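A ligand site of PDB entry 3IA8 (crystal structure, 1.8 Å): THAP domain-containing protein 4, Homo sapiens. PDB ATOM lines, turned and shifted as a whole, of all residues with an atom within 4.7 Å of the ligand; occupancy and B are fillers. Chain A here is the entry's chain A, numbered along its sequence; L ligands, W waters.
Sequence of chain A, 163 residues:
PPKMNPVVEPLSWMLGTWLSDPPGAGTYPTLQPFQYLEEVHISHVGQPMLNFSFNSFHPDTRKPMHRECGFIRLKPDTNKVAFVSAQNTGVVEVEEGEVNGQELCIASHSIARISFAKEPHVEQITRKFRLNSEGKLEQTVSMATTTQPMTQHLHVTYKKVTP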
ATOM      1  N   TYR A  28      10.298 -16.934   7.187  1.00  0.00           N
ATOM      2  CA  TYR A  28      10.786 -16.043   6.144  1.00  0.00           C
ATOM      3  C   TYR A  28      11.846 -15.147   6.795  1.00  0.00           C
ATOM      4  O   TYR A  28      11.810 -14.943   8.002  1.00  0.00           O
ATOM      5  CB  TYR A  28       9.656 -15.224   5.514  1.00  0.00           C
ATOM      6  CG  TYR A  28       9.870 -14.970   4.031  1.00  0.00           C
ATOM      7  CD1 TYR A  28      10.099 -16.028   3.162  1.00  0.00           C
ATOM      8  CD2 TYR A  28       9.826 -13.673   3.513  1.00  0.00           C
ATOM      9  CE1 TYR A  28      10.283 -15.824   1.813  1.00  0.00           C
ATOM     10  CE2 TYR A  28      10.028 -13.455   2.144  1.00  0.00           C
ATOM     11  CZ  TYR A  28      10.255 -14.532   1.306  1.00  0.00           C
ATOM     12  OH  TYR A  28      10.463 -14.345  -0.033  1.00  0.00           O
ATOM     13  N   THR A  30      12.050 -12.221   7.074  1.00  0.00           N
ATOM     14  CA  THR A  30      11.394 -11.055   7.662  1.00  0.00           C
ATOM     15  C   THR A  30      10.424 -11.378   8.802  1.00  0.00           C
ATOM     16  O   THR A  30       9.873 -10.475   9.419  1.00  0.00           O
ATOM     17  CB  THR A  30      10.604 -10.294   6.586  1.00  0.00           C
ATOM     18  OG1 THR A  30       9.683 -11.204   5.961  1.00  0.00           O
ATOM     19  CG2 THR A  30      11.522  -9.749   5.542  1.00  0.00           C
ATOM     20  N   LEU A  31      10.234 -12.665   9.088  1.00  0.00           N
ATOM     21  CA  LEU A  31       9.138 -13.109   9.965  1.00  0.00           C
ATOM     22  C   LEU A  31       9.658 -13.923  11.137  1.00  0.00           C
ATOM     23  O   LEU A  31      10.623 -14.661  11.006  1.00  0.00           O
ATOM     24  CB  LEU A  31       8.150 -14.005   9.200  1.00  0.00           C
ATOM     25  CG  LEU A  31       7.477 -13.419   7.954  1.00  0.00           C
ATOM     26  CD1 LEU A  31       6.477 -14.438   7.368  1.00  0.00           C
ATOM     27  CD2 LEU A  31       6.770 -12.087   8.292  1.00  0.00           C
ATOM     28  N   PHE A  34       6.694 -19.462  12.700  1.00  0.00           N
ATOM     29  CA  PHE A  34       5.360 -19.707  13.211  1.00  0.00           C
ATOM     30  C   PHE A  34       4.940 -21.132  12.880  1.00  0.00           C
ATOM     31  O   PHE A  34       5.607 -21.796  12.089  1.00  0.00           O
ATOM     32  CB  PHE A  34       4.353 -18.681  12.689  1.00  0.00           C
ATOM     33  CG  PHE A  34       4.200 -18.677  11.180  1.00  0.00           C
ATOM     34  CD1 PHE A  34       4.976 -17.863  10.401  1.00  0.00           C
ATOM     35  CD2 PHE A  34       3.250 -19.478  10.568  1.00  0.00           C
ATOM     36  CE1 PHE A  34       4.822 -17.827   9.031  1.00  0.00           C
ATOM     37  CE2 PHE A  34       3.091 -19.463   9.194  1.00  0.00           C
ATOM     38  CZ  PHE A  34       3.880 -18.640   8.419  1.00  0.00           C
ATOM     39  N   TYR A  36       1.331 -23.674  11.987  1.00  0.00           N
ATOM     40  CA  TYR A  36      -0.068 -23.591  11.569  1.00  0.00           C
ATOM     41  C   TYR A  36      -0.641 -24.979  11.363  1.00  0.00           C
ATOM     42  O   TYR A  36       0.104 -25.931  11.153  1.00  0.00           O
ATOM     43  CB  TYR A  36      -0.214 -22.772  10.303  1.00  0.00           C
ATOM     44  CG  TYR A  36       0.527 -23.327   9.112  1.00  0.00           C
ATOM     45  CD1 TYR A  36       1.877 -23.067   8.936  1.00  0.00           C
ATOM     46  CD2 TYR A  36      -0.133 -24.085   8.134  1.00  0.00           C
ATOM     47  CE1 TYR A  36       2.557 -23.545   7.829  1.00  0.00           C
ATOM     48  CE2 TYR A  36       0.540 -24.568   7.034  1.00  0.00           C
ATOM     49  CZ  TYR A  36       1.880 -24.306   6.894  1.00  0.00           C
ATOM     50  OH  TYR A  36       2.567 -24.779   5.797  1.00  0.00           O
ATOM     51  N   GLU A  38      -3.213 -27.285   8.979  1.00  0.00           N
ATOM     52  CA  GLU A  38      -3.744 -27.177   7.615  1.00  0.00           C
ATOM     53  C   GLU A  38      -4.524 -28.432   7.265  1.00  0.00           C
ATOM     54  O   GLU A  38      -4.086 -29.562   7.543  1.00  0.00           O
ATOM     55  CB  GLU A  38      -2.618 -26.927   6.597  1.00  0.00           C
ATOM     56  CG  GLU A  38      -3.130 -26.624   5.166  1.00  0.00           C
ATOM     57  CD  GLU A  38      -2.008 -26.256   4.205  1.00  0.00           C
ATOM     58  OE1 GLU A  38      -0.881 -26.769   4.360  1.00  0.00           O
ATOM     59  OE2 GLU A  38      -2.258 -25.462   3.260  1.00  0.00           O
ATOM     60  N   SER A  56      -5.713 -23.323   6.038  1.00  0.00           N
ATOM     61  CA  SER A  56      -4.888 -23.273   7.231  1.00  0.00           C
ATOM     62  C   SER A  56      -5.584 -22.556   8.371  1.00  0.00           C
ATOM     63  O   SER A  56      -6.477 -21.721   8.140  1.00  0.00           O
ATOM     64  CB  SER A  56      -3.552 -22.589   6.941  1.00  0.00           C
ATOM     65  OG  SER A  56      -2.897 -23.188   5.839  1.00  0.00           O
ATOM     66  N   MET A  65      -6.756 -18.930   8.585  1.00  0.00           N
ATOM     67  CA  MET A  65      -5.672 -18.082   8.102  1.00  0.00           C
ATOM     68  C   MET A  65      -5.630 -18.176   6.584  1.00  0.00           C
ATOM     69  O   MET A  65      -6.612 -17.866   5.926  1.00  0.00           O
ATOM     70  CB  MET A  65      -4.353 -18.458   8.780  1.00  0.00           C
ATOM     71  CG  MET A  65      -4.408 -18.219  10.290  1.00  0.00           C
ATOM     72  SD  MET A  65      -2.833 -18.789  11.250  1.00  0.00           S
ATOM     73  CE  MET A  65      -1.609 -17.402  10.716  1.00  0.00           C
ATOM     74  N   HIS A  66      -4.511 -18.644   6.022  1.00  0.00           N
ATOM     75  CA  HIS A  66      -4.398 -18.748   4.562  1.00  0.00           C
ATOM     76  C   HIS A  66      -5.414 -19.769   4.018  1.00  0.00           C
ATOM     77  O   HIS A  66      -5.677 -20.801   4.668  1.00  0.00           O
ATOM     78  CB  HIS A  66      -2.986 -19.202   4.193  1.00  0.00           C
ATOM     79  CG  HIS A  66      -2.686 -19.175   2.715  1.00  0.00           C
ATOM     80  ND1 HIS A  66      -2.669 -20.314   1.933  1.00  0.00           N
ATOM     81  CD2 HIS A  66      -2.348 -18.149   1.906  1.00  0.00           C
ATOM     82  CE1 HIS A  66      -2.355 -19.975   0.695  1.00  0.00           C
ATOM     83  NE2 HIS A  66      -2.153 -18.673   0.651  1.00  0.00           N
ATOM     84  N   GLU A  68      -6.596 -21.503  -0.010  1.00  0.00           N
ATOM     85  CA  GLU A  68      -6.473 -21.461  -1.458  1.00  0.00           C
ATOM     86  C   GLU A  68      -7.216 -22.645  -2.055  1.00  0.00           C
ATOM     87  O   GLU A  68      -7.495 -23.618  -1.367  1.00  0.00           O
ATOM     88  CB  GLU A  68      -5.000 -21.457  -1.881  1.00  0.00           C
ATOM     89  CG  GLU A  68      -4.175 -22.594  -1.354  1.00  0.00           C
ATOM     90  CD  GLU A  68      -2.732 -22.558  -1.886  1.00  0.00           C
ATOM     91  OE1 GLU A  68      -2.524 -22.269  -3.087  1.00  0.00           O
ATOM     92  OE2 GLU A  68      -1.812 -22.826  -1.108  1.00  0.00           O
ATOM     93  N   GLN A  87      -6.031 -17.618  -4.130  1.00  0.00           N
ATOM     94  CA  GLN A  87      -5.703 -17.541  -2.710  1.00  0.00           C
ATOM     95  C   GLN A  87      -6.468 -16.408  -2.032  1.00  0.00           C
ATOM     96  O   GLN A  87      -6.764 -15.391  -2.655  1.00  0.00           O
ATOM     97  CB  GLN A  87      -4.189 -17.323  -2.546  1.00  0.00           C
ATOM     98  CG  GLN A  87      -3.418 -18.346  -3.400  1.00  0.00           C
ATOM     99  CD  GLN A  87      -1.938 -18.317  -3.179  1.00  0.00           C
ATOM    100  OE1 GLN A  87      -1.446 -17.599  -2.332  1.00  0.00           O
ATOM    101  NE2 GLN A  87      -1.217 -19.133  -3.931  1.00  0.00           N
ATOM    102  N   GLU A  93      -2.337 -17.626  -9.235  1.00  0.00           N
ATOM    103  CA  GLU A  93      -1.038 -18.020  -9.798  1.00  0.00           C
ATOM    104  C   GLU A  93      -1.205 -19.235 -10.689  1.00  0.00           C
ATOM    105  O   GLU A  93      -2.153 -20.017 -10.517  1.00  0.00           O
ATOM    106  CB  GLU A  93      -0.074 -18.330  -8.667  1.00  0.00           C
ATOM    107  CG  GLU A  93      -0.575 -19.462  -7.803  1.00  0.00           C
ATOM    108  CD  GLU A  93       0.498 -20.116  -6.987  1.00  0.00           C
ATOM    109  OE1 GLU A  93       1.646 -20.228  -7.459  1.00  0.00           O
ATOM    110  OE2 GLU A  93       0.185 -20.530  -5.854  1.00  0.00           O
ATOM    111  N   PRO A 120       4.252  -7.034   1.486  1.00  0.00           N
ATOM    112  CA  PRO A 120       4.922  -7.102   0.172  1.00  0.00           C
ATOM    113  C   PRO A 120       4.258  -8.095  -0.766  1.00  0.00           C
ATOM    114  O   PRO A 120       3.780  -9.138  -0.313  1.00  0.00           O
ATOM    115  CB  PRO A 120       6.309  -7.659   0.501  1.00  0.00           C
ATOM    116  CG  PRO A 120       6.365  -7.851   1.968  1.00  0.00           C
ATOM    117  CD  PRO A 120       4.979  -7.795   2.505  1.00  0.00           C
ATOM    118  N   HIS A 121       4.299  -7.811  -2.058  1.00  0.00           N
ATOM    119  CA  HIS A 121       3.743  -8.728  -3.060  1.00  0.00           C
ATOM    120  C   HIS A 121       4.680  -9.890  -3.382  1.00  0.00           C
ATOM    121  O   HIS A 121       5.885  -9.714  -3.578  1.00  0.00           O
ATOM    122  CB  HIS A 121       3.428  -7.959  -4.346  1.00  0.00           C
ATOM    123  CG  HIS A 121       2.512  -6.790  -4.149  1.00  0.00           C
ATOM    124  ND1 HIS A 121       1.443  -6.809  -3.274  1.00  0.00           N
ATOM    125  CD2 HIS A 121       2.503  -5.562  -4.724  1.00  0.00           C
ATOM    126  CE1 HIS A 121       0.820  -5.646  -3.324  1.00  0.00           C
ATOM    127  NE2 HIS A 121       1.446  -4.868  -4.183  1.00  0.00           N
ATOM    128  N   VAL A 122       4.107 -11.088  -3.497  1.00  0.00           N
ATOM    129  CA  VAL A 122       4.891 -12.235  -3.960  1.00  0.00           C
ATOM    130  C   VAL A 122       5.137 -12.124  -5.461  1.00  0.00           C
ATOM    131  O   VAL A 122       4.239 -11.736  -6.203  1.00  0.00           O
ATOM    132  CB  VAL A 122       4.213 -13.582  -3.611  1.00  0.00           C
ATOM    133  CG1 VAL A 122       2.877 -13.719  -4.335  1.00  0.00           C
ATOM    134  CG2 VAL A 122       5.128 -14.750  -3.941  1.00  0.00           C
ATOM    135  N   ILE A 125       6.791 -18.157  -6.924  1.00  0.00           N
ATOM    136  CA  ILE A 125       6.502 -19.210  -5.955  1.00  0.00           C
ATOM    137  C   ILE A 125       7.014 -20.521  -6.541  1.00  0.00           C
ATOM    138  O   ILE A 125       6.917 -20.741  -7.744  1.00  0.00           O
ATOM    139  CB  ILE A 125       4.950 -19.363  -5.712  1.00  0.00           C
ATOM    140  CG1 ILE A 125       4.323 -18.045  -5.253  1.00  0.00           C
ATOM    141  CG2 ILE A 125       4.643 -20.472  -4.691  1.00  0.00           C
ATOM    142  CD1 ILE A 125       2.779 -18.051  -5.323  1.00  0.00           C
ATOM    143  N   ARG A 127       6.835 -24.854  -5.501  1.00  0.00           N
ATOM    144  CA  ARG A 127       6.359 -25.831  -4.546  1.00  0.00           C
ATOM    145  C   ARG A 127       6.918 -27.189  -4.884  1.00  0.00           C
ATOM    146  O   ARG A 127       7.142 -27.521  -6.051  1.00  0.00           O
ATOM    147  CB  ARG A 127       4.842 -25.913  -4.568  1.00  0.00           C
ATOM    148  CG  ARG A 127       4.123 -24.569  -4.514  1.00  0.00           C
ATOM    149  CD  ARG A 127       2.673 -24.807  -4.131  1.00  0.00           C
ATOM    150  NE  ARG A 127       1.840 -23.628  -4.328  1.00  0.00           N
ATOM    151  CZ  ARG A 127       0.796 -23.298  -3.578  1.00  0.00           C
ATOM    152  NH1 ARG A 127       0.423 -24.056  -2.556  1.00  0.00           N
ATOM    153  NH2 ARG A 127       0.111 -22.204  -3.861  1.00  0.00           N
ATOM    154  N   VAL A 141       7.048 -24.937   0.272  1.00  0.00           N
ATOM    155  CA  VAL A 141       6.757 -23.792  -0.575  1.00  0.00           C
ATOM    156  C   VAL A 141       7.870 -22.777  -0.379  1.00  0.00           C
ATOM    157  O   VAL A 141       8.214 -22.443   0.760  1.00  0.00           O
ATOM    158  CB  VAL A 141       5.397 -23.163  -0.183  1.00  0.00           C
ATOM    159  CG1 VAL A 141       5.085 -21.896  -1.001  1.00  0.00           C
ATOM    160  CG2 VAL A 141       4.260 -24.197  -0.293  1.00  0.00           C
ATOM    161  N   MET A 143       9.309 -18.805  -1.981  1.00  0.00           N
ATOM    162  CA  MET A 143       8.811 -17.635  -2.685  1.00  0.00           C
ATOM    163  C   MET A 143       9.815 -16.504  -2.660  1.00  0.00           C
ATOM    164  O   MET A 143      10.640 -16.417  -1.755  1.00  0.00           O
ATOM    165  CB  MET A 143       7.493 -17.160  -2.102  1.00  0.00           C
ATOM    166  CG  MET A 143       7.628 -16.499  -0.734  1.00  0.00           C
ATOM    167  SD  MET A 143       5.893 -16.216   0.053  1.00  0.00           S
ATOM    168  CE  MET A 143       6.508 -15.351   1.710  1.00  0.00           C
ATOM    169  N   THR A 145       9.672 -12.268  -2.908  1.00  0.00           N
ATOM    170  CA  THR A 145       8.774 -11.137  -2.896  1.00  0.00           C
ATOM    171  C   THR A 145       9.476  -9.969  -3.545  1.00  0.00           C
ATOM    172  O   THR A 145      10.611 -10.099  -4.027  1.00  0.00           O
ATOM    173  CB  THR A 145       8.376 -10.749  -1.464  1.00  0.00           C
ATOM    174  OG1 THR A 145       9.517 -10.186  -0.805  1.00  0.00           O
ATOM    175  CG2 THR A 145       7.856 -11.971  -0.704  1.00  0.00           C
ATOM    176  N   HIS A 153       9.324 -20.616   2.549  1.00  0.00           N
ATOM    177  CA  HIS A 153       8.290 -19.977   3.370  1.00  0.00           C
ATOM    178  C   HIS A 153       7.535 -21.003   4.225  1.00  0.00           C
ATOM    179  O   HIS A 153       7.206 -20.702   5.382  1.00  0.00           O
ATOM    180  CB  HIS A 153       7.299 -19.213   2.473  1.00  0.00           C
ATOM    181  CG  HIS A 153       6.195 -18.528   3.218  1.00  0.00           C
ATOM    182  ND1 HIS A 153       6.389 -17.816   4.389  1.00  0.00           N
ATOM    183  CD2 HIS A 153       4.875 -18.382   2.909  1.00  0.00           C
ATOM    184  CE1 HIS A 153       5.237 -17.290   4.782  1.00  0.00           C
ATOM    185  NE2 HIS A 153       4.309 -17.624   3.910  1.00  0.00           N
ATOM    186  N   LEU A 154       7.282 -22.179   3.667  1.00  0.00           N
ATOM    187  CA  LEU A 154       6.445 -23.173   4.336  1.00  0.00           C
ATOM    188  C   LEU A 154       7.030 -24.576   4.185  1.00  0.00           C
ATOM    189  O   LEU A 154       7.565 -24.915   3.113  1.00  0.00           O
ATOM    190  CB  LEU A 154       5.035 -23.200   3.735  1.00  0.00           C
ATOM    191  CG  LEU A 154       4.260 -21.885   3.587  1.00  0.00           C
ATOM    192  CD1 LEU A 154       2.977 -22.149   2.784  1.00  0.00           C
ATOM    193  CD2 LEU A 154       3.960 -21.298   4.966  1.00  0.00           C
HETATM  194  C1  LIG L   1       3.396 -13.731   5.219  1.00  0.00           C
HETATM  195  C2  LIG L   1       2.775 -15.219   0.659  1.00  0.00           C
HETATM  196  C3  LIG L   1       0.935 -19.406   2.406  1.00  0.00           C
HETATM  197  C4  LIG L   1       0.965 -17.659   6.931  1.00  0.00           C
HETATM  198  C5  LIG L   1       3.414 -13.773   3.846  1.00  0.00           C
HETATM  199  C6  LIG L   1       3.985 -12.773   2.990  1.00  0.00           C
HETATM  200  C7  LIG L   1       3.797 -13.170   1.727  1.00  0.00           C
HETATM  201  C8  LIG L   1       3.126 -14.456   1.752  1.00  0.00           C
HETATM  202  C9  LIG L   1       4.212 -12.440   0.429  1.00  0.00           C
HETATM  203  C10 LIG L   1       4.612 -11.464   3.533  1.00  0.00           C
HETATM  204  C11 LIG L   1       6.133 -11.613   3.604  1.00  0.00           C
HETATM  205  C12 LIG L   1       6.738 -10.503   4.431  1.00  0.00           C
HETATM  206  O1  LIG L   1       7.890 -10.138   4.101  1.00  0.00           O
HETATM  207  O2  LIG L   1       6.097  -9.996   5.399  1.00  0.00           O
HETATM  208  C13 LIG L   1       2.246 -16.492   0.743  1.00  0.00           C
HETATM  209  C14 LIG L   1       2.027 -17.405  -0.372  1.00  0.00           C
HETATM  210  C15 LIG L   1       1.503 -18.548   0.110  1.00  0.00           C
HETATM  211  C16 LIG L   1       1.422 -18.422   1.554  1.00  0.00           C
HETATM  212  C17 LIG L   1       2.292 -17.089  -1.859  1.00  0.00           C
HETATM  213  C18 LIG L   1       1.096 -19.822  -0.675  1.00  0.00           C
HETATM  214  C19 LIG L   1       1.778 -20.212  -1.754  1.00  0.00           C
HETATM  215  C20 LIG L   1       0.747 -19.310   3.764  1.00  0.00           C
HETATM  216  C21 LIG L   1       0.165 -20.318   4.651  1.00  0.00           C
HETATM  217  C22 LIG L   1       0.167 -19.828   5.911  1.00  0.00           C
HETATM  218  C23 LIG L   1       0.759 -18.502   5.857  1.00  0.00           C
HETATM  219  C24 LIG L   1      -0.363 -21.697   4.224  1.00  0.00           C
HETATM  220  C25 LIG L   1      -0.362 -20.543   7.162  1.00  0.00           C
HETATM  221  C26 LIG L   1      -0.916 -19.845   8.166  1.00  0.00           C
HETATM  222  C27 LIG L   1       1.639 -16.457   6.871  1.00  0.00           C
HETATM  223  C28 LIG L   1       1.917 -15.607   8.013  1.00  0.00           C
HETATM  224  C29 LIG L   1       2.670 -14.413   7.456  1.00  0.00           C
HETATM  225  C30 LIG L   1       2.770 -14.631   6.045  1.00  0.00           C
HETATM  226  C31 LIG L   1       1.550 -15.855   9.484  1.00  0.00           C
HETATM  227  C32 LIG L   1       3.224 -13.174   8.186  1.00  0.00           C
HETATM  228  C33 LIG L   1       2.035 -12.401   8.748  1.00  0.00           C
HETATM  229  C34 LIG L   1       2.649 -11.223   9.464  1.00  0.00           C
HETATM  230  O3  LIG L   1       3.229 -10.340   8.778  1.00  0.00           O
HETATM  231  O4  LIG L   1       2.541 -11.191  10.720  1.00  0.00           O
HETATM  232  N1  LIG L   1       2.916 -14.800   3.078  1.00  0.00           N
HETATM  233  N2  LIG L   1       1.878 -17.144   1.897  1.00  0.00           N
HETATM  234  N3  LIG L   1       1.108 -18.242   4.556  1.00  0.00           N
HETATM  235  N4  LIG L   1       2.161 -15.843   5.726  1.00  0.00           N
HETATM  236 FE1  LIG L   1       2.271 -16.637   3.840  1.00  0.00          FE
HETATM  237  O   HOH W   1       9.395  -9.963   1.847  1.00  0.00           O
HETATM  238  O   HOH W   2       5.536  -8.932   9.720  1.00  0.00           O
HETATM  239  O   HOH W   3       0.844 -13.315  -1.323  1.00  0.00           O
HETATM  240  O   HOH W   4       3.721  -9.674   6.352  1.00  0.00           O
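An iron atom (FE1) of the ligand is bound by a ring nitrogen (NE2) of His 153, at 2.3 Å. An oxygen (O1) of the ligand sits at hydrogen-bond distance from the side-chain hydroxyl of Thr 30 (2.8 Å).
A ring nitrogen (NE2) of His 66 lies within hydrogen-bond range of the side-chain amide oxygen of Gln 87, 3.2 Å away. The side-chain amide nitrogen of Gln 87 lies within hydrogen-bond range of the side-chain carboxylate of Glu 93 (2.8 Å). N of Met 65 sits at hydrogen-bond distance from O of Ser 56, 2.8 Å away. The side-chain carboxylate (OE1) of Glu 68 lies within salt-bridge range of the guanidinium group (NH2) of Arg 127 (2.7 Å). The side-chain carboxylate (OE2) of Glu 93 lies within salt-bridge range of the guanidinium group (NH2) of Arg 127 (2.6 Å). O of His 66 is in hydrogen-bond range of N of Ser 56. NH2 of Arg 127 sits close to NE2 of Gln 87, at 3.3 Å. The backbone NH (N) of His 153 sits at hydrogen-bond distance from the backbone carbonyl oxygen (O) of Val 141, at 2.8 Å.
Leu 31 touches the ligand. CZ of Phe 34 touches C4 of the ligand, 3.4 Å away. Tyr 36 touches the ligand. OG of Ser 56 touches C24 of the ligand, at 3.4 Å. Met 65 touches the ligand. His 66 touches the ligand. Gln 87 touches the ligand (OE1 to C18, 3.8 Å). O of Pro 120 touches C9 of the ligand, 3.4 Å away. Ile 125 touches the ligand (CD1 to C17, 3.6 Å). Arg 127 touches the ligand (NH2 to C19, 3.3 Å). CG1 of Val 141 touches C19 of the ligand, 3.8 Å away. SD of Met 143 touches C2 of the ligand, 3.3 Å away. Thr 145 touches the ligand (CG2 to C9, 3.8 Å). CD1 of Leu 154 touches C3 of the ligand, at 3.4 Å. Within 4 Å of the ligand: Thr 30, Leu 31, Phe 34, Tyr 36, Ser 56, Met 65, His 66, Gln 87, Pro 120, Ile 125, Arg 127, Val 141, Met 143, Thr 145, His 153 and Leu 154.
Water W1 bridges the side-chain hydroxyl (OG1) of Thr 145 (2.7 Å) and an oxygen (O1) of the ligand (2.7 Å).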
